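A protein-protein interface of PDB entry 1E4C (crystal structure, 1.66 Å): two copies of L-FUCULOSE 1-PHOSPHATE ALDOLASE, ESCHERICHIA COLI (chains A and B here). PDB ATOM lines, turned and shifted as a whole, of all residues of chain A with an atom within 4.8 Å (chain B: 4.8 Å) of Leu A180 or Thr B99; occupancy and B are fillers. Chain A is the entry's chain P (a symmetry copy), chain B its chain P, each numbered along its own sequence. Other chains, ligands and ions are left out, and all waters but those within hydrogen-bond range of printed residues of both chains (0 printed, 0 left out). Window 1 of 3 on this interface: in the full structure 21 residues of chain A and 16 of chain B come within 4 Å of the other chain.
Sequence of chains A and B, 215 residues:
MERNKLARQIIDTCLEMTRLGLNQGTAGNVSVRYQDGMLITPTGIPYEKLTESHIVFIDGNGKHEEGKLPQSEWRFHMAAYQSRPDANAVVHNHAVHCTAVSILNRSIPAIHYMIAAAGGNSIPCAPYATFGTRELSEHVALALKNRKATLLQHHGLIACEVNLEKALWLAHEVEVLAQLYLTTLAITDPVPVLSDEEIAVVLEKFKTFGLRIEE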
ATOM      1  N   ILE A 111     -18.385  13.440  23.008  1.00  0.00           N
ATOM      2  CA  ILE A 111     -19.445  13.753  22.054  1.00  0.00           C
ATOM      3  C   ILE A 111     -20.604  14.527  22.684  1.00  0.00           C
ATOM      4  O   ILE A 111     -21.516  15.033  22.031  1.00  0.00           O
ATOM      5  CB  ILE A 111     -19.976  12.464  21.404  1.00  0.00           C
ATOM      6  CG1 ILE A 111     -20.551  11.491  22.442  1.00  0.00           C
ATOM      7  CG2 ILE A 111     -18.871  11.795  20.589  1.00  0.00           C
ATOM      8  CD1 ILE A 111     -21.334  10.362  21.787  1.00  0.00           C
ATOM      9  N   HIS A 112     -20.635  14.577  23.999  1.00  0.00           N
ATOM     10  CA  HIS A 112     -21.686  15.217  24.780  1.00  0.00           C
ATOM     11  C   HIS A 112     -21.074  15.688  26.090  1.00  0.00           C
ATOM     12  O   HIS A 112     -20.143  15.032  26.581  1.00  0.00           O
ATOM     13  CB  HIS A 112     -22.823  14.221  25.006  1.00  0.00           C
ATOM     14  CG  HIS A 112     -24.070  14.852  25.547  1.00  0.00           C
ATOM     15  ND1 HIS A 112     -24.190  15.228  26.862  1.00  0.00           N
ATOM     16  CD2 HIS A 112     -25.244  15.177  24.935  1.00  0.00           C
ATOM     17  CE1 HIS A 112     -25.384  15.782  27.053  1.00  0.00           C
ATOM     18  NE2 HIS A 112     -26.045  15.738  25.905  1.00  0.00           N
ATOM     19  N   VAL A 176     -26.382   5.658  27.665  1.00  0.00           N
ATOM     20  CA  VAL A 176     -26.910   6.698  26.780  1.00  0.00           C
ATOM     21  C   VAL A 176     -25.794   7.252  25.893  1.00  0.00           C
ATOM     22  O   VAL A 176     -25.968   7.413  24.674  1.00  0.00           O
ATOM     23  CB  VAL A 176     -27.591   7.841  27.560  1.00  0.00           C
ATOM     24  CG1 VAL A 176     -27.947   9.014  26.652  1.00  0.00           C
ATOM     25  CG2 VAL A 176     -28.862   7.280  28.203  1.00  0.00           C
ATOM     26  N   LEU A 177     -24.636   7.523  26.490  1.00  0.00           N
ATOM     27  CA  LEU A 177     -23.502   8.024  25.697  1.00  0.00           C
ATOM     28  C   LEU A 177     -23.051   7.035  24.634  1.00  0.00           C
ATOM     29  O   LEU A 177     -22.712   7.415  23.512  1.00  0.00           O
ATOM     30  CB  LEU A 177     -22.313   8.317  26.622  1.00  0.00           C
ATOM     31  CG  LEU A 177     -22.419   9.606  27.431  1.00  0.00           C
ATOM     32  CD1 LEU A 177     -21.459   9.543  28.611  1.00  0.00           C
ATOM     33  CD2 LEU A 177     -22.164  10.852  26.591  1.00  0.00           C
ATOM     34  N   ALA A 178     -23.048   5.733  24.967  1.00  0.00           N
ATOM     35  CA  ALA A 178     -22.679   4.692  24.014  1.00  0.00           C
ATOM     36  C   ALA A 178     -23.678   4.617  22.864  1.00  0.00           C
ATOM     37  O   ALA A 178     -23.320   4.479  21.700  1.00  0.00           O
ATOM     38  CB  ALA A 178     -22.599   3.331  24.700  1.00  0.00           C
ATOM     39  N   GLN A 179     -24.973   4.749  23.170  1.00  0.00           N
ATOM     40  CA  GLN A 179     -25.991   4.754  22.124  1.00  0.00           C
ATOM     41  C   GLN A 179     -25.819   5.976  21.237  1.00  0.00           C
ATOM     42  O   GLN A 179     -25.911   5.886  20.017  1.00  0.00           O
ATOM     43  CB  GLN A 179     -27.397   4.676  22.731  1.00  0.00           C
ATOM     44  CG  GLN A 179     -28.453   4.525  21.649  1.00  0.00           C
ATOM     45  CD  GLN A 179     -29.873   4.385  22.154  1.00  0.00           C
ATOM     46  OE1 GLN A 179     -30.082   4.436  23.367  1.00  0.00           O
ATOM     47  NE2 GLN A 179     -30.809   4.221  21.210  1.00  0.00           N
ATOM     48  N   LEU A 180     -25.543   7.153  21.821  1.00  0.00           N
ATOM     49  CA  LEU A 180     -25.322   8.352  21.013  1.00  0.00           C
ATOM     50  C   LEU A 180     -24.132   8.168  20.075  1.00  0.00           C
ATOM     51  O   LEU A 180     -24.162   8.542  18.899  1.00  0.00           O
ATOM     52  CB  LEU A 180     -25.045   9.549  21.928  1.00  0.00           C
ATOM     53  CG  LEU A 180     -26.257  10.034  22.727  1.00  0.00           C
ATOM     54  CD1 LEU A 180     -25.738  11.043  23.737  1.00  0.00           C
ATOM     55  CD2 LEU A 180     -27.291  10.655  21.793  1.00  0.00           C
ATOM     56  N   TYR A 181     -23.066   7.561  20.597  1.00  0.00           N
ATOM     57  CA  TYR A 181     -21.851   7.321  19.813  1.00  0.00           C
ATOM     58  C   TYR A 181     -22.080   6.351  18.660  1.00  0.00           C
ATOM     59  O   TYR A 181     -21.692   6.624  17.524  1.00  0.00           O
ATOM     60  CB  TYR A 181     -20.734   6.801  20.735  1.00  0.00           C
ATOM     61  CG  TYR A 181     -19.349   6.809  20.109  1.00  0.00           C
ATOM     62  CD1 TYR A 181     -18.954   7.839  19.271  1.00  0.00           C
ATOM     63  CD2 TYR A 181     -18.454   5.787  20.397  1.00  0.00           C
ATOM     64  CE1 TYR A 181     -17.683   7.845  18.712  1.00  0.00           C
ATOM     65  CE2 TYR A 181     -17.183   5.784  19.847  1.00  0.00           C
ATOM     66  CZ  TYR A 181     -16.819   6.823  19.009  1.00  0.00           C
ATOM     67  OH  TYR A 181     -15.552   6.814  18.453  1.00  0.00           O
ATOM     68  N   LEU A 182     -22.709   5.199  18.921  1.00  0.00           N
ATOM     69  CA  LEU A 182     -22.947   4.250  17.834  1.00  0.00           C
ATOM     70  C   LEU A 182     -23.895   4.802  16.776  1.00  0.00           C
ATOM     71  O   LEU A 182     -23.744   4.462  15.588  1.00  0.00           O
ATOM     72  CB  LEU A 182     -23.532   2.958  18.422  1.00  0.00           C
ATOM     73  CG  LEU A 182     -22.576   2.173  19.322  1.00  0.00           C
ATOM     74  CD1 LEU A 182     -23.400   1.268  20.225  1.00  0.00           C
ATOM     75  CD2 LEU A 182     -21.578   1.387  18.477  1.00  0.00           C
ATOM     76  N   THR A 183     -24.905   5.557  17.200  1.00  0.00           N
ATOM     77  CA  THR A 183     -25.897   6.087  16.268  1.00  0.00           C
ATOM     78  C   THR A 183     -25.264   7.101  15.322  1.00  0.00           C
ATOM     79  O   THR A 183     -25.569   7.111  14.129  1.00  0.00           O
ATOM     80  CB  THR A 183     -27.059   6.732  17.050  1.00  0.00           C
ATOM     81  OG1 THR A 183     -27.650   5.694  17.857  1.00  0.00           O
ATOM     82  CG2 THR A 183     -28.105   7.303  16.118  1.00  0.00           C
ATOM     83  N   THR A 184     -24.368   7.916  15.861  1.00  0.00           N
ATOM     84  CA  THR A 184     -23.685   8.931  15.071  1.00  0.00           C
ATOM     85  C   THR A 184     -22.522   8.330  14.288  1.00  0.00           C
ATOM     86  O   THR A 184     -22.341   8.757  13.134  1.00  0.00           O
ATOM     87  CB  THR A 184     -23.219  10.108  15.945  1.00  0.00           C
ATOM     88  OG1 THR A 184     -22.448   9.639  17.058  1.00  0.00           O
ATOM     89  CG2 THR A 184     -24.439  10.872  16.475  1.00  0.00           C
ATOM     90  N   HIS B  94     -32.875  15.360  27.099  1.00  0.00           N
ATOM     91  CA  HIS B  94     -31.727  14.917  26.322  1.00  0.00           C
ATOM     92  C   HIS B  94     -32.168  13.621  25.609  1.00  0.00           C
ATOM     93  O   HIS B  94     -31.450  12.632  25.622  1.00  0.00           O
ATOM     94  CB  HIS B  94     -30.485  14.679  27.169  1.00  0.00           C
ATOM     95  CG  HIS B  94     -29.977  15.857  27.946  1.00  0.00           C
ATOM     96  ND1 HIS B  94     -28.891  15.711  28.784  1.00  0.00           N
ATOM     97  CD2 HIS B  94     -30.340  17.163  28.020  1.00  0.00           C
ATOM     98  CE1 HIS B  94     -28.629  16.885  29.357  1.00  0.00           C
ATOM     99  NE2 HIS B  94     -29.497  17.782  28.906  1.00  0.00           N
ATOM    100  N   ALA B  95     -33.351  13.643  24.997  1.00  0.00           N
ATOM    101  CA  ALA B  95     -33.861  12.454  24.300  1.00  0.00           C
ATOM    102  C   ALA B  95     -32.829  11.988  23.280  1.00  0.00           C
ATOM    103  O   ALA B  95     -32.185  12.801  22.627  1.00  0.00           O
ATOM    104  CB  ALA B  95     -35.208  12.770  23.674  1.00  0.00           C
ATOM    105  N   VAL B  96     -32.637  10.676  23.185  1.00  0.00           N
ATOM    106  CA  VAL B  96     -31.503  10.131  22.435  1.00  0.00           C
ATOM    107  C   VAL B  96     -31.461  10.489  20.973  1.00  0.00           C
ATOM    108  O   VAL B  96     -30.377  10.887  20.496  1.00  0.00           O
ATOM    109  CB  VAL B  96     -31.402   8.607  22.673  1.00  0.00           C
ATOM    110  CG1 VAL B  96     -32.398   7.802  21.866  1.00  0.00           C
ATOM    111  CG2 VAL B  96     -29.983   8.134  22.384  1.00  0.00           C
ATOM    112  N   HIS B  97     -32.555  10.390  20.215  1.00  0.00           N
ATOM    113  CA  HIS B  97     -32.474  10.718  18.786  1.00  0.00           C
ATOM    114  C   HIS B  97     -32.277  12.197  18.556  1.00  0.00           C
ATOM    115  O   HIS B  97     -31.410  12.605  17.749  1.00  0.00           O
ATOM    116  CB  HIS B  97     -33.696  10.144  18.042  1.00  0.00           C
ATOM    117  CG  HIS B  97     -33.699   8.646  18.200  1.00  0.00           C
ATOM    118  ND1 HIS B  97     -34.481   8.009  19.138  1.00  0.00           N
ATOM    119  CD2 HIS B  97     -33.021   7.673  17.531  1.00  0.00           C
ATOM    120  CE1 HIS B  97     -34.270   6.704  19.054  1.00  0.00           C
ATOM    121  NE2 HIS B  97     -33.389   6.470  18.091  1.00  0.00           N
ATOM    122  N   CYS B  98     -33.001  13.054  19.280  1.00  0.00           N
ATOM    123  CA  CYS B  98     -32.812  14.495  19.180  1.00  0.00           C
ATOM    124  C   CYS B  98     -31.350  14.855  19.477  1.00  0.00           C
ATOM    125  O   CYS B  98     -30.706  15.637  18.777  1.00  0.00           O
ATOM    126  CB  CYS B  98     -33.640  15.252  20.212  1.00  0.00           C
ATOM    127  SG  CYS B  98     -35.395  15.324  19.806  1.00  0.00           S
ATOM    128  N   THR B  99     -30.836  14.235  20.531  1.00  0.00           N
ATOM    129  CA  THR B  99     -29.455  14.523  20.957  1.00  0.00           C
ATOM    130  C   THR B  99     -28.424  14.049  19.951  1.00  0.00           C
ATOM    131  O   THR B  99     -27.431  14.751  19.717  1.00  0.00           O
ATOM    132  CB  THR B  99     -29.239  13.938  22.362  1.00  0.00           C
ATOM    133  OG1 THR B  99     -30.254  14.530  23.199  1.00  0.00           O
ATOM    134  CG2 THR B  99     -27.878  14.314  22.925  1.00  0.00           C
ATOM    135  N   ALA B 100     -28.629  12.886  19.342  1.00  0.00           N
ATOM    136  CA  ALA B 100     -27.707  12.413  18.304  1.00  0.00           C
ATOM    137  C   ALA B 100     -27.720  13.368  17.121  1.00  0.00           C
ATOM    138  O   ALA B 100     -26.648  13.671  16.575  1.00  0.00           O
ATOM    139  CB  ALA B 100     -28.066  11.005  17.840  1.00  0.00           C
ATOM    140  N   VAL B 101     -28.911  13.864  16.708  1.00  0.00           N
ATOM    141  CA  VAL B 101     -28.891  14.828  15.595  1.00  0.00           C
ATOM    142  C   VAL B 101     -28.137  16.081  16.018  1.00  0.00           C
ATOM    143  O   VAL B 101     -27.359  16.629  15.212  1.00  0.00           O
ATOM    144  CB  VAL B 101     -30.306  15.187  15.110  1.00  0.00           C
ATOM    145  CG1 VAL B 101     -30.229  16.247  14.012  1.00  0.00           C
ATOM    146  CG2 VAL B 101     -31.014  13.934  14.604  1.00  0.00           C
ATOM    147  N   SER B 102     -28.271  16.496  17.290  1.00  0.00           N
ATOM    148  CA  SER B 102     -27.559  17.687  17.767  1.00  0.00           C
ATOM    149  C   SER B 102     -26.040  17.520  17.798  1.00  0.00           C
ATOM    150  O   SER B 102     -25.300  18.520  17.712  1.00  0.00           O
ATOM    151  CB  SER B 102     -28.050  18.046  19.181  1.00  0.00           C
ATOM    152  OG  SER B 102     -27.282  17.434  20.196  1.00  0.00           O
ATOM    153  N   ILE B 103     -25.561  16.277  17.860  1.00  0.00           N
ATOM    154  CA  ILE B 103     -24.114  16.019  17.851  1.00  0.00           C
ATOM    155  C   ILE B 103     -23.567  16.196  16.444  1.00  0.00           C
ATOM    156  O   ILE B 103     -22.453  16.692  16.244  1.00  0.00           O
ATOM    157  CB  ILE B 103     -23.839  14.619  18.416  1.00  0.00           C
ATOM    158  CG1 ILE B 103     -24.080  14.663  19.931  1.00  0.00           C
ATOM    159  CG2 ILE B 103     -22.404  14.196  18.128  1.00  0.00           C
ATOM    160  CD1 ILE B 103     -24.155  13.287  20.567  1.00  0.00           C
ATOM    161  N   HIS B 155     -26.087  18.585  23.074  1.00  0.00           N
ATOM    162  CA  HIS B 155     -26.806  18.733  24.345  1.00  0.00           C
ATOM    163  C   HIS B 155     -28.163  18.058  24.332  1.00  0.00           C
ATOM    164  O   HIS B 155     -28.343  17.087  25.083  1.00  0.00           O
ATOM    165  CB  HIS B 155     -26.909  20.239  24.654  1.00  0.00           C
ATOM    166  CG  HIS B 155     -27.481  20.531  26.016  1.00  0.00           C
ATOM    167  ND1 HIS B 155     -27.163  21.666  26.725  1.00  0.00           N
ATOM    168  CD2 HIS B 155     -28.337  19.842  26.789  1.00  0.00           C
ATOM    169  CE1 HIS B 155     -27.819  21.636  27.886  1.00  0.00           C
ATOM    170  NE2 HIS B 155     -28.545  20.526  27.952  1.00  0.00           N
ATOM    171  N   GLY B 156     -29.132  18.566  23.573  1.00  0.00           N
ATOM    172  CA  GLY B 156     -30.468  17.954  23.668  1.00  0.00           C
ATOM    173  C   GLY B 156     -31.511  18.814  22.965  1.00  0.00           C
ATOM    174  O   GLY B 156     -31.257  19.367  21.901  1.00  0.00           O
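Of the printed residues of chain B, Leu A180 touches Val B96, Thr B99 and Ala B100. Thr B99 touches two residues of chain A. Of the printed residues of chain A, His B94 touches His A112. Printed residues of chain A within 4 Å of His B155: His A112. Printed residues of chain A within 4 Å of Ile B103: Ile A111 (3.3 Å). The nearest printed residue of chain A that does not touch Val B96 is Val A176 (4.7 Å).
The backbone carbonyl oxygen (O) of His B155 is in hydrogen-bond range of a ring nitrogen (NE2) of His A112 (2.8 Å).
The backbone carbonyl oxygen of Leu A180 sits at hydrogen-bond distance from the side-chain hydroxyl of Thr A184 (2.7 Å). O of Tyr A181 is in hydrogen-bond range of OG1 of Thr A184 (3.1 Å). OG of Ser B102 sits at hydrogen-bond distance from N of His B155, 3.3 Å away. O of Ala B95 sits at hydrogen-bond distance from OG1 of Thr B99. The backbone carbonyl oxygen (O) of His B94 lies close to the side-chain hydroxyl (OG1) of Thr B99 (3.3 Å). The backbone carbonyl oxygen (O) of Gln A179 is in hydrogen-bond range of the side-chain hydroxyl (OG1) of Thr A183 (2.8 Å).
Among the printed residues, pairs that only touch across the chains: Ile A111 with Ile B103 (3.3 Å), Leu A180 with Val B96 (3.4 Å), His A112 with Thr B99 (3.4 Å), Thr A184 with Ala B100 (3.6 Å), Leu A180 with Ala B100 (3.6 Å), Gln A179 with Val B96 (3.8 Å), Leu A180 with Thr B99 (3.9 Å) and His A112 with His B94 (3.9 Å).
Printed residues of chain A that touch a printed residue of chain B: Ile A111, His A112, Gln A179, Leu A180 and Thr A184. Hydrophobic or aromatic side chains of chain A that line the printed part of chain B: His A112 and Leu A180. Among the printed residues, no Asp or Glu carboxylate lies within 4 Å of a Lys or Arg side-chain nitrogen of the other chain.
No position is printed for both chains. Of the 9 pairs that touch across the chains among the printed residues, none has its exchanged pair printed and touching as well.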
